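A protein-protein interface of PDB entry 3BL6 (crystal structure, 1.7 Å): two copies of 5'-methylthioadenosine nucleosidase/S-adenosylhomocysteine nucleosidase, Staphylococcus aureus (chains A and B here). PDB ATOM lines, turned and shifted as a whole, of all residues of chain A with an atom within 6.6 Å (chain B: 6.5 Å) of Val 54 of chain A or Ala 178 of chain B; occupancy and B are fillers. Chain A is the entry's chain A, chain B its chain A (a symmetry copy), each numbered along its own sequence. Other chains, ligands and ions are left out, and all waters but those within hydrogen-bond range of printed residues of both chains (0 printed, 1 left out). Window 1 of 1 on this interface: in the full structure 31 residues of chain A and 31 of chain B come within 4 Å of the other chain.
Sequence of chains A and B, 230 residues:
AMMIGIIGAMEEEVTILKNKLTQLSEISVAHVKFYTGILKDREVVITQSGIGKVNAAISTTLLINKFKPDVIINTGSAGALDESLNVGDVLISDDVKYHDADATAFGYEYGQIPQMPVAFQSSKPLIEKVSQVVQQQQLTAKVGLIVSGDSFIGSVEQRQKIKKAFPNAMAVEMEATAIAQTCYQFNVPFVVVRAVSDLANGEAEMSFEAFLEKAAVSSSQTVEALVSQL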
ATOM      1  N   SER A  49     -21.844 -30.496  17.237  1.00  0.00           N
ATOM      2  CA  SER A  49     -22.821 -30.062  16.240  1.00  0.00           C
ATOM      3  C   SER A  49     -22.398 -29.274  15.009  1.00  0.00           C
ATOM      4  O   SER A  49     -23.087 -29.313  13.988  1.00  0.00           O
ATOM      5  CB  SER A  49     -23.903 -29.244  16.936  1.00  0.00           C
ATOM      6  OG  SER A  49     -23.370 -28.020  17.414  1.00  0.00           O
ATOM      7  N   ILE A  51     -21.174 -25.311  13.663  1.00  0.00           N
ATOM      8  CA  ILE A  51     -21.624 -23.962  14.005  1.00  0.00           C
ATOM      9  C   ILE A  51     -22.886 -23.464  13.302  1.00  0.00           C
ATOM     10  O   ILE A  51     -23.170 -23.849  12.164  1.00  0.00           O
ATOM     11  CB  ILE A  51     -20.466 -22.957  13.740  1.00  0.00           C
ATOM     12  CG1 ILE A  51     -19.255 -23.334  14.602  1.00  0.00           C
ATOM     13  CG2 ILE A  51     -20.909 -21.527  14.033  1.00  0.00           C
ATOM     14  CD1 ILE A  51     -17.925 -22.729  14.167  1.00  0.00           C
ATOM     15  N   GLY A  52     -23.637 -22.605  13.994  1.00  0.00           N
ATOM     16  CA  GLY A  52     -24.842 -22.030  13.419  1.00  0.00           C
ATOM     17  C   GLY A  52     -26.161 -22.744  13.664  1.00  0.00           C
ATOM     18  O   GLY A  52     -26.199 -23.886  14.130  1.00  0.00           O
ATOM     19  N   LYS A  53     -27.248 -22.067  13.301  1.00  0.00           N
ATOM     20  CA  LYS A  53     -28.605 -22.567  13.504  1.00  0.00           C
ATOM     21  C   LYS A  53     -28.933 -23.922  12.894  1.00  0.00           C
ATOM     22  O   LYS A  53     -29.458 -24.807  13.573  1.00  0.00           O
ATOM     23  CB  LYS A  53     -29.627 -21.558  12.967  1.00  0.00           C
ATOM     24  CG  LYS A  53     -29.627 -20.197  13.626  1.00  0.00           C
ATOM     25  CD  LYS A  53     -30.844 -19.399  13.130  1.00  0.00           C
ATOM     26  CE  LYS A  53     -30.844 -17.985  13.650  1.00  0.00           C
ATOM     27  NZ  LYS A  53     -32.019 -17.216  13.112  1.00  0.00           N
ATOM     28  N   VAL A  54     -28.637 -24.078  11.610  1.00  0.00           N
ATOM     29  CA  VAL A  54     -28.965 -25.319  10.922  1.00  0.00           C
ATOM     30  C   VAL A  54     -28.125 -26.498  11.405  1.00  0.00           C
ATOM     31  O   VAL A  54     -28.659 -27.591  11.618  1.00  0.00           O
ATOM     32  CB  VAL A  54     -28.867 -25.121   9.381  1.00  0.00           C
ATOM     33  CG1 VAL A  54     -29.029 -26.451   8.643  1.00  0.00           C
ATOM     34  CG2 VAL A  54     -29.971 -24.154   8.934  1.00  0.00           C
ATOM     35  N   ASN A  55     -26.823 -26.297  11.599  1.00  0.00           N
ATOM     36  CA  ASN A  55     -26.000 -27.407  12.085  1.00  0.00           C
ATOM     37  C   ASN A  55     -26.498 -27.840  13.463  1.00  0.00           C
ATOM     38  O   ASN A  55     -26.574 -29.038  13.757  1.00  0.00           O
ATOM     39  CB  ASN A  55     -24.516 -27.016  12.156  1.00  0.00           C
ATOM     40  CG  ASN A  55     -23.853 -27.044  10.793  1.00  0.00           C
ATOM     41  OD1 ASN A  55     -24.260 -27.811   9.923  1.00  0.00           O
ATOM     42  ND2 ASN A  55     -22.825 -26.217  10.601  1.00  0.00           N
ATOM     43  N   ALA A  56     -26.854 -26.866  14.296  1.00  0.00           N
ATOM     44  CA  ALA A  56     -27.360 -27.158  15.639  1.00  0.00           C
ATOM     45  C   ALA A  56     -28.683 -27.911  15.578  1.00  0.00           C
ATOM     46  O   ALA A  56     -28.896 -28.850  16.339  1.00  0.00           O
ATOM     47  CB  ALA A  56     -27.536 -25.862  16.441  1.00  0.00           C
ATOM     48  N   ALA A  57     -29.572 -27.492  14.679  1.00  0.00           N
ATOM     49  CA  ALA A  57     -30.876 -28.142  14.532  1.00  0.00           C
ATOM     50  C   ALA A  57     -30.732 -29.582  14.048  1.00  0.00           C
ATOM     51  O   ALA A  57     -31.386 -30.485  14.563  1.00  0.00           O
ATOM     52  CB  ALA A  57     -31.745 -27.361  13.564  1.00  0.00           C
ATOM     53  N   ILE A  58     -29.935 -29.791  13.101  1.00  0.00           N
ATOM     54  CA  ILE A  58     -29.678 -31.126  12.581  1.00  0.00           C
ATOM     55  C   ILE A  58     -29.148 -32.012  13.702  1.00  0.00           C
ATOM     56  O   ILE A  58     -29.644 -33.116  13.919  1.00  0.00           O
ATOM     57  CB  ILE A  58     -28.626 -31.103  11.442  1.00  0.00           C
ATOM     58  CG1 ILE A  58     -29.160 -30.309  10.240  1.00  0.00           C
ATOM     59  CG2 ILE A  58     -28.291 -32.543  11.027  1.00  0.00           C
ATOM     60  CD1 ILE A  58     -28.146 -29.985   9.103  1.00  0.00           C
ATOM     61  N   SER A  59     -28.109 -31.550  14.340  1.00  0.00           N
ATOM     62  CA  SER A  59     -27.502 -32.304  15.435  1.00  0.00           C
ATOM     63  C   SER A  59     -28.480 -32.609  16.558  1.00  0.00           C
ATOM     64  O   SER A  59     -28.526 -33.731  17.059  1.00  0.00           O
ATOM     65  CB  SER A  59     -26.301 -31.532  16.004  1.00  0.00           C
ATOM     66  OG  SER A  59     -25.287 -31.409  15.027  1.00  0.00           O
ATOM     67  N   ASP A 150     -27.169 -16.199  13.172  1.00  0.00           N
ATOM     68  CA  ASP A 150     -26.218 -16.900  12.304  1.00  0.00           C
ATOM     69  C   ASP A 150     -25.075 -15.948  11.952  1.00  0.00           C
ATOM     70  O   ASP A 150     -24.516 -16.000  10.852  1.00  0.00           O
ATOM     71  CB  ASP A 150     -26.857 -17.427  11.012  1.00  0.00           C
ATOM     72  CG  ASP A 150     -27.217 -18.901  11.092  1.00  0.00           C
ATOM     73  OD1 ASP A 150     -26.795 -19.573  12.063  1.00  0.00           O
ATOM     74  OD2 ASP A 150     -27.908 -19.395  10.173  1.00  0.00           O
ATOM     75  N   MET A 174     -24.270 -18.510  18.539  1.00  0.00           N
ATOM     76  CA  MET A 174     -24.975 -19.007  17.365  1.00  0.00           C
ATOM     77  C   MET A 174     -25.920 -20.201  17.369  1.00  0.00           C
ATOM     78  O   MET A 174     -26.732 -20.330  16.458  1.00  0.00           O
ATOM     79  CB  MET A 174     -23.863 -19.039  16.297  1.00  0.00           C
ATOM     80  CG  MET A 174     -23.167 -17.689  16.097  1.00  0.00           C
ATOM     81  SD  MET A 174     -21.673 -17.723  15.032  1.00  0.00           S
ATOM     82  CE  MET A 174     -22.388 -18.136  13.434  1.00  0.00           C
ATOM     83  N   ALA A 178     -31.512 -22.267  18.441  1.00  0.00           N
ATOM     84  CA  ALA A 178     -31.837 -23.296  17.446  1.00  0.00           C
ATOM     85  C   ALA A 178     -32.024 -24.631  18.170  1.00  0.00           C
ATOM     86  O   ALA A 178     -32.928 -25.398  17.868  1.00  0.00           O
ATOM     87  CB  ALA A 178     -30.703 -23.412  16.400  1.00  0.00           C
ATOM     88  N   GLY B  52     -38.975 -20.891   8.397  1.00  0.00           N
ATOM     89  CA  GLY B  52     -37.640 -20.586   8.885  1.00  0.00           C
ATOM     90  C   GLY B  52     -36.588 -21.681   8.819  1.00  0.00           C
ATOM     91  O   GLY B  52     -36.892 -22.853   8.580  1.00  0.00           O
ATOM     92  N   LYS B  53     -35.343 -21.288   9.076  1.00  0.00           N
ATOM     93  CA  LYS B  53     -34.192 -22.184   9.010  1.00  0.00           C
ATOM     94  C   LYS B  53     -34.249 -23.434   9.877  1.00  0.00           C
ATOM     95  O   LYS B  53     -34.019 -24.545   9.394  1.00  0.00           O
ATOM     96  CB  LYS B  53     -32.909 -21.427   9.374  1.00  0.00           C
ATOM     97  CG  LYS B  53     -32.538 -20.275   8.467  1.00  0.00           C
ATOM     98  CD  LYS B  53     -31.130 -19.779   8.836  1.00  0.00           C
ATOM     99  CE  LYS B  53     -30.740 -18.552   8.056  1.00  0.00           C
ATOM    100  NZ  LYS B  53     -29.379 -18.063   8.470  1.00  0.00           N
ATOM    101  N   VAL B  54     -34.541 -23.250  11.159  1.00  0.00           N
ATOM    102  CA  VAL B  54     -34.563 -24.378  12.079  1.00  0.00           C
ATOM    103  C   VAL B  54     -35.719 -25.336  11.807  1.00  0.00           C
ATOM    104  O   VAL B  54     -35.526 -26.557  11.822  1.00  0.00           O
ATOM    105  CB  VAL B  54     -34.556 -23.870  13.551  1.00  0.00           C
ATOM    106  CG1 VAL B  54     -34.762 -25.024  14.534  1.00  0.00           C
ATOM    107  CG2 VAL B  54     -33.209 -23.193  13.836  1.00  0.00           C
ATOM    108  N   ALA B  56     -37.123 -25.870   9.005  1.00  0.00           N
ATOM    109  CA  ALA B  56     -36.760 -26.546   7.758  1.00  0.00           C
ATOM    110  C   ALA B  56     -35.707 -27.620   7.998  1.00  0.00           C
ATOM    111  O   ALA B  56     -35.793 -28.708   7.437  1.00  0.00           O
ATOM    112  CB  ALA B  56     -36.243 -25.533   6.728  1.00  0.00           C
ATOM    113  N   ALA B  57     -34.709 -27.310   8.826  1.00  0.00           N
ATOM    114  CA  ALA B  57     -33.643 -28.265   9.131  1.00  0.00           C
ATOM    115  C   ALA B  57     -34.180 -29.483   9.876  1.00  0.00           C
ATOM    116  O   ALA B  57     -33.827 -30.617   9.562  1.00  0.00           O
ATOM    117  CB  ALA B  57     -32.559 -27.596   9.955  1.00  0.00           C
ATOM    118  N   THR B  60     -36.250 -31.533   7.365  1.00  0.00           N
ATOM    119  CA  THR B  60     -35.425 -32.229   6.379  1.00  0.00           C
ATOM    120  C   THR B  60     -34.631 -33.379   7.009  1.00  0.00           C
ATOM    121  O   THR B  60     -34.504 -34.442   6.414  1.00  0.00           O
ATOM    122  CB  THR B  60     -34.469 -31.253   5.684  1.00  0.00           C
ATOM    123  OG1 THR B  60     -35.232 -30.144   5.198  1.00  0.00           O
ATOM    124  CG2 THR B  60     -33.763 -31.926   4.491  1.00  0.00           C
ATOM    125  N   THR B  61     -34.111 -33.163   8.213  1.00  0.00           N
ATOM    126  CA  THR B  61     -33.352 -34.193   8.915  1.00  0.00           C
ATOM    127  C   THR B  61     -34.240 -35.425   9.152  1.00  0.00           C
ATOM    128  O   THR B  61     -33.827 -36.556   8.888  1.00  0.00           O
ATOM    129  CB  THR B  61     -32.824 -33.653  10.269  1.00  0.00           C
ATOM    130  OG1 THR B  61     -31.932 -32.559  10.023  1.00  0.00           O
ATOM    131  CG2 THR B  61     -32.079 -34.736  11.040  1.00  0.00           C
ATOM    132  N   VAL B  96     -27.684 -21.845  -3.797  1.00  0.00           N
ATOM    133  CA  VAL B  96     -28.416 -21.144  -2.740  1.00  0.00           C
ATOM    134  C   VAL B  96     -27.415 -20.725  -1.668  1.00  0.00           C
ATOM    135  O   VAL B  96     -26.426 -21.413  -1.440  1.00  0.00           O
ATOM    136  CB  VAL B  96     -29.526 -22.012  -2.112  1.00  0.00           C
ATOM    137  CG1 VAL B  96     -30.564 -22.369  -3.179  1.00  0.00           C
ATOM    138  CG2 VAL B  96     -28.924 -23.263  -1.476  1.00  0.00           C
ATOM    139  N   TYR B  98     -27.059 -18.107   2.214  1.00  0.00           N
ATOM    140  CA  TYR B  98     -27.741 -17.329   3.248  1.00  0.00           C
ATOM    141  C   TYR B  98     -27.388 -15.864   3.010  1.00  0.00           C
ATOM    142  O   TYR B  98     -26.240 -15.548   2.720  1.00  0.00           O
ATOM    143  CB  TYR B  98     -27.241 -17.718   4.642  1.00  0.00           C
ATOM    144  CG  TYR B  98     -27.618 -19.105   5.078  1.00  0.00           C
ATOM    145  CD1 TYR B  98     -28.959 -19.489   5.165  1.00  0.00           C
ATOM    146  CD2 TYR B  98     -26.639 -20.035   5.423  1.00  0.00           C
ATOM    147  CE1 TYR B  98     -29.316 -20.766   5.581  1.00  0.00           C
ATOM    148  CE2 TYR B  98     -26.986 -21.320   5.842  1.00  0.00           C
ATOM    149  CZ  TYR B  98     -28.328 -21.678   5.913  1.00  0.00           C
ATOM    150  OH  TYR B  98     -28.660 -22.962   6.283  1.00  0.00           O
ATOM    151  N   PHE B 120     -24.635 -23.739  -1.505  1.00  0.00           N
ATOM    152  CA  PHE B 120     -25.005 -25.109  -1.794  1.00  0.00           C
ATOM    153  C   PHE B 120     -25.583 -25.249  -3.199  1.00  0.00           C
ATOM    154  O   PHE B 120     -26.201 -24.333  -3.704  1.00  0.00           O
ATOM    155  CB  PHE B 120     -25.964 -25.631  -0.719  1.00  0.00           C
ATOM    156  CG  PHE B 120     -25.405 -25.512   0.668  1.00  0.00           C
ATOM    157  CD1 PHE B 120     -24.533 -26.464   1.152  1.00  0.00           C
ATOM    158  CD2 PHE B 120     -25.709 -24.428   1.464  1.00  0.00           C
ATOM    159  CE1 PHE B 120     -23.990 -26.343   2.392  1.00  0.00           C
ATOM    160  CE2 PHE B 120     -25.159 -24.307   2.719  1.00  0.00           C
ATOM    161  CZ  PHE B 120     -24.304 -25.273   3.178  1.00  0.00           C
ATOM    162  N   SER B 148     -31.546 -17.255   1.331  1.00  0.00           N
ATOM    163  CA  SER B 148     -32.433 -17.501   2.465  1.00  0.00           C
ATOM    164  C   SER B 148     -31.966 -16.771   3.725  1.00  0.00           C
ATOM    165  O   SER B 148     -30.798 -16.442   3.871  1.00  0.00           O
ATOM    166  CB  SER B 148     -32.569 -18.992   2.756  1.00  0.00           C
ATOM    167  OG  SER B 148     -32.764 -19.725   1.573  1.00  0.00           O
ATOM    168  N   MET B 174     -37.324 -18.095   3.173  1.00  0.00           N
ATOM    169  CA  MET B 174     -36.758 -18.540   4.440  1.00  0.00           C
ATOM    170  C   MET B 174     -36.195 -19.932   4.690  1.00  0.00           C
ATOM    171  O   MET B 174     -35.429 -20.112   5.632  1.00  0.00           O
ATOM    172  CB  MET B 174     -37.802 -18.047   5.462  1.00  0.00           C
ATOM    173  CG  MET B 174     -38.076 -16.542   5.382  1.00  0.00           C
ATOM    174  SD  MET B 174     -39.487 -15.943   6.390  1.00  0.00           S
ATOM    175  CE  MET B 174     -38.875 -16.231   8.058  1.00  0.00           C
ATOM    176  N   GLU B 175     -36.539 -20.912   3.857  1.00  0.00           N
ATOM    177  CA  GLU B 175     -36.025 -22.258   4.099  1.00  0.00           C
ATOM    178  C   GLU B 175     -35.052 -22.952   3.154  1.00  0.00           C
ATOM    179  O   GLU B 175     -34.272 -23.795   3.584  1.00  0.00           O
ATOM    180  CB  GLU B 175     -37.306 -23.114   4.181  1.00  0.00           C
ATOM    181  CG  GLU B 175     -38.336 -22.641   5.236  1.00  0.00           C
ATOM    182  CD  GLU B 175     -39.310 -21.600   4.707  1.00  0.00           C
ATOM    183  OE1 GLU B 175     -39.460 -21.474   3.471  1.00  0.00           O
ATOM    184  OE2 GLU B 175     -39.938 -20.910   5.535  1.00  0.00           O
ATOM    185  N   ALA B 176     -35.097 -22.601   1.875  1.00  0.00           N
ATOM    186  CA  ALA B 176     -34.271 -23.266   0.868  1.00  0.00           C
ATOM    187  C   ALA B 176     -32.834 -23.575   1.236  1.00  0.00           C
ATOM    188  O   ALA B 176     -32.387 -24.715   1.096  1.00  0.00           O
ATOM    189  CB  ALA B 176     -34.309 -22.479  -0.450  1.00  0.00           C
ATOM    190  N   THR B 177     -32.097 -22.573   1.696  1.00  0.00           N
ATOM    191  CA  THR B 177     -30.699 -22.802   2.031  1.00  0.00           C
ATOM    192  C   THR B 177     -30.528 -23.737   3.235  1.00  0.00           C
ATOM    193  O   THR B 177     -29.564 -24.511   3.281  1.00  0.00           O
ATOM    194  CB  THR B 177     -29.975 -21.466   2.270  1.00  0.00           C
ATOM    195  OG1 THR B 177     -30.177 -20.614   1.132  1.00  0.00           O
ATOM    196  CG2 THR B 177     -28.470 -21.701   2.434  1.00  0.00           C
ATOM    197  N   ALA B 178     -31.462 -23.678   4.191  1.00  0.00           N
ATOM    198  CA  ALA B 178     -31.417 -24.547   5.373  1.00  0.00           C
ATOM    199  C   ALA B 178     -31.641 -25.992   4.923  1.00  0.00           C
ATOM    200  O   ALA B 178     -30.986 -26.914   5.391  1.00  0.00           O
ATOM    201  CB  ALA B 178     -32.507 -24.131   6.390  1.00  0.00           C
ATOM    202  N   ILE B 179     -32.611 -26.174   4.019  1.00  0.00           N
ATOM    203  CA  ILE B 179     -32.864 -27.490   3.455  1.00  0.00           C
ATOM    204  C   ILE B 179     -31.630 -27.947   2.674  1.00  0.00           C
ATOM    205  O   ILE B 179     -31.209 -29.104   2.771  1.00  0.00           O
ATOM    206  CB  ILE B 179     -34.091 -27.431   2.525  1.00  0.00           C
ATOM    207  CG1 ILE B 179     -35.331 -27.069   3.353  1.00  0.00           C
ATOM    208  CG2 ILE B 179     -34.298 -28.766   1.822  1.00  0.00           C
ATOM    209  CD1 ILE B 179     -36.536 -26.752   2.623  1.00  0.00           C
ATOM    210  N   ALA B 180     -31.056 -27.096   1.911  1.00  0.00           N
ATOM    211  CA  ALA B 180     -29.881 -27.441   1.108  1.00  0.00           C
ATOM    212  C   ALA B 180     -28.691 -27.817   1.992  1.00  0.00           C
ATOM    213  O   ALA B 180     -27.947 -28.754   1.686  1.00  0.00           O
ATOM    214  CB  ALA B 180     -29.506 -26.268   0.190  1.00  0.00           C
ATOM    215  N   GLN B 181     -28.503 -27.077   3.080  1.00  0.00           N
ATOM    216  CA  GLN B 181     -27.406 -27.357   3.994  1.00  0.00           C
ATOM    217  C   GLN B 181     -27.596 -28.733   4.609  1.00  0.00           C
ATOM    218  O   GLN B 181     -26.631 -29.491   4.798  1.00  0.00           O
ATOM    219  CB  GLN B 181     -27.348 -26.311   5.113  1.00  0.00           C
ATOM    220  CG  GLN B 181     -26.180 -26.538   6.066  1.00  0.00           C
ATOM    221  CD  GLN B 181     -26.044 -25.453   7.112  1.00  0.00           C
ATOM    222  OE1 GLN B 181     -26.527 -24.333   6.933  1.00  0.00           O
ATOM    223  NE2 GLN B 181     -25.370 -25.778   8.209  1.00  0.00           N
ATOM    224  N   THR B 182     -28.842 -29.057   4.926  1.00  0.00           N
ATOM    225  CA  THR B 182     -29.146 -30.357   5.516  1.00  0.00           C
ATOM    226  C   THR B 182     -28.877 -31.458   4.485  1.00  0.00           C
ATOM    227  O   THR B 182     -28.285 -32.493   4.809  1.00  0.00           O
ATOM    228  CB  THR B 182     -30.610 -30.411   5.995  1.00  0.00           C
ATOM    229  OG1 THR B 182     -30.844 -29.342   6.926  1.00  0.00           O
ATOM    230  CG2 THR B 182     -30.890 -31.735   6.694  1.00  0.00           C
ATOM    231  N   CYS B 183     -29.283 -31.223   3.240  1.00  0.00           N
ATOM    232  CA  CYS B 183     -29.051 -32.201   2.182  1.00  0.00           C
ATOM    233  C   CYS B 183     -27.558 -32.355   1.937  1.00  0.00           C
ATOM    234  O   CYS B 183     -27.088 -33.438   1.586  1.00  0.00           O
ATOM    235  CB  CYS B 183     -29.768 -31.787   0.890  1.00  0.00           C
ATOM    236  SG  CYS B 183     -31.576 -31.993   0.936  1.00  0.00           S
ATOM    237  N   GLN B 185     -25.210 -32.067   4.263  1.00  0.00           N
ATOM    238  CA  GLN B 185     -24.710 -32.893   5.359  1.00  0.00           C
ATOM    239  C   GLN B 185     -25.027 -34.382   5.183  1.00  0.00           C
ATOM    240  O   GLN B 185     -24.250 -35.226   5.621  1.00  0.00           O
ATOM    241  CB  GLN B 185     -25.234 -32.377   6.704  1.00  0.00           C
ATOM    242  CG  GLN B 185     -24.716 -30.972   7.082  1.00  0.00           C
ATOM    243  CD  GLN B 185     -23.205 -30.906   7.319  1.00  0.00           C
ATOM    244  OE1 GLN B 185     -22.408 -31.316   6.473  1.00  0.00           O
ATOM    245  NE2 GLN B 185     -22.809 -30.373   8.473  1.00  0.00           N
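OD1 of Asn 55 of chain A lies within hydrogen-bond range of NE2 of Gln 181 of chain B, 2.9 Å away. The side-chain amide oxygen (OD1) of Asn 55 of chain A sits at hydrogen-bond distance from the side-chain amide nitrogen (NE2) of Gln 185 of chain B, at 3.3 Å. OD2 of Asp 150 of chain A is in salt-bridge range of NZ of Lys 53 of chain B, 2.6 Å away.
O of Ile 51 of chain A lies within hydrogen-bond range of ND2 of Asn 55 of chain A. N of Lys 53 of chain A sits at hydrogen-bond distance from OD1 of Asp 150 of chain A, 2.8 Å away. The backbone carbonyl oxygen (O) of Asn 55 of chain A sits at hydrogen-bond distance from the side-chain hydroxyl (OG) of Ser 59 of chain A, at 3.0 Å. The side-chain hydroxyl of Thr 61 of chain B is in hydrogen-bond range of the backbone carbonyl oxygen of Ala 57 of chain B (2.8 Å). The side-chain hydroxyl (OH) of Tyr 98 of chain B is in hydrogen-bond range of the side-chain amide oxygen (OE1) of Gln 181 of chain B, 2.6 Å away. O of Ala 178 of chain B lies within hydrogen-bond range of OG1 of Thr 182 of chain B (2.9 Å).
Among the printed residues, merely in contact across the chains: Val 54 of chain A with Tyr 98 of chain B (3.2 Å), Val 54 of chain A with Gln 181 of chain B (3.5 Å), Ile 58 of chain A with Thr 182 of chain B (3.5 Å), Ile 58 of chain A with Thr 61 of chain B (3.6 Å), Ala 178 of chain A with Val 54 of chain B (3.6 Å), Val 54 of chain A with Ala 178 of chain B (3.6 Å), Ala 57 of chain A with Ala 57 of chain B (3.7 Å), Val 54 of chain A with Thr 182 of chain B (3.8 Å), Val 54 of chain A with Ala 57 of chain B (3.9 Å) and Ala 57 of chain A with Val 54 of chain B (3.9 Å).
Val 54 of chain A touches just these residues of chain B: Ala 57 (3.9 Å), Tyr 98 (3.2 Å), Ala 178 (3.6 Å), Gln 181 (3.5 Å) and Thr 182 (3.8 Å). Of the printed residues of chain A, Ala 178 of chain B touches Val 54. Of the printed residues of chain A, Thr 61 of chain B touches Ile 58 (3.6 Å). Printed residues of chain A within 4 Å of Val 54 of chain B: Ala 57 (3.9 Å) and Ala 178 (3.6 Å).
Hydrophobic or aromatic side chains of chain B within 4 Å of the printed part of chain A: Val 54, Ala 57, Tyr 98 and Ala 178. Of the 13 printed residues of chain A, 6 touch a printed residue of chain B. Hydrophobic or aromatic side chains of chain A that line the printed part of chain B: Val 54, Ala 57, Ile 58 and Ala 178. Among the printed residues, 13 pairs touch across the chains. Among the printed residues, Asp or Glu carboxylates within 4 Å of a Lys or Arg side-chain nitrogen of the other chain: Asp 150 of chain A with Lys 53 of chain B (2.6 Å).
Val 54 of chain A touches Ala 57 of chain B, and with the chains exchanged Ala 57 of chain A touches Val 54 of chain B. Val 54 of chain A touches Ala 178 of chain B, and with the chains exchanged Ala 178 of chain A touches Val 54 of chain B. Ala 57 of chain B touches its own counterpart, Ala 57 of chain A. Positions printed for both chains: 52, 53, 54, 56, 57, 174 and 178.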
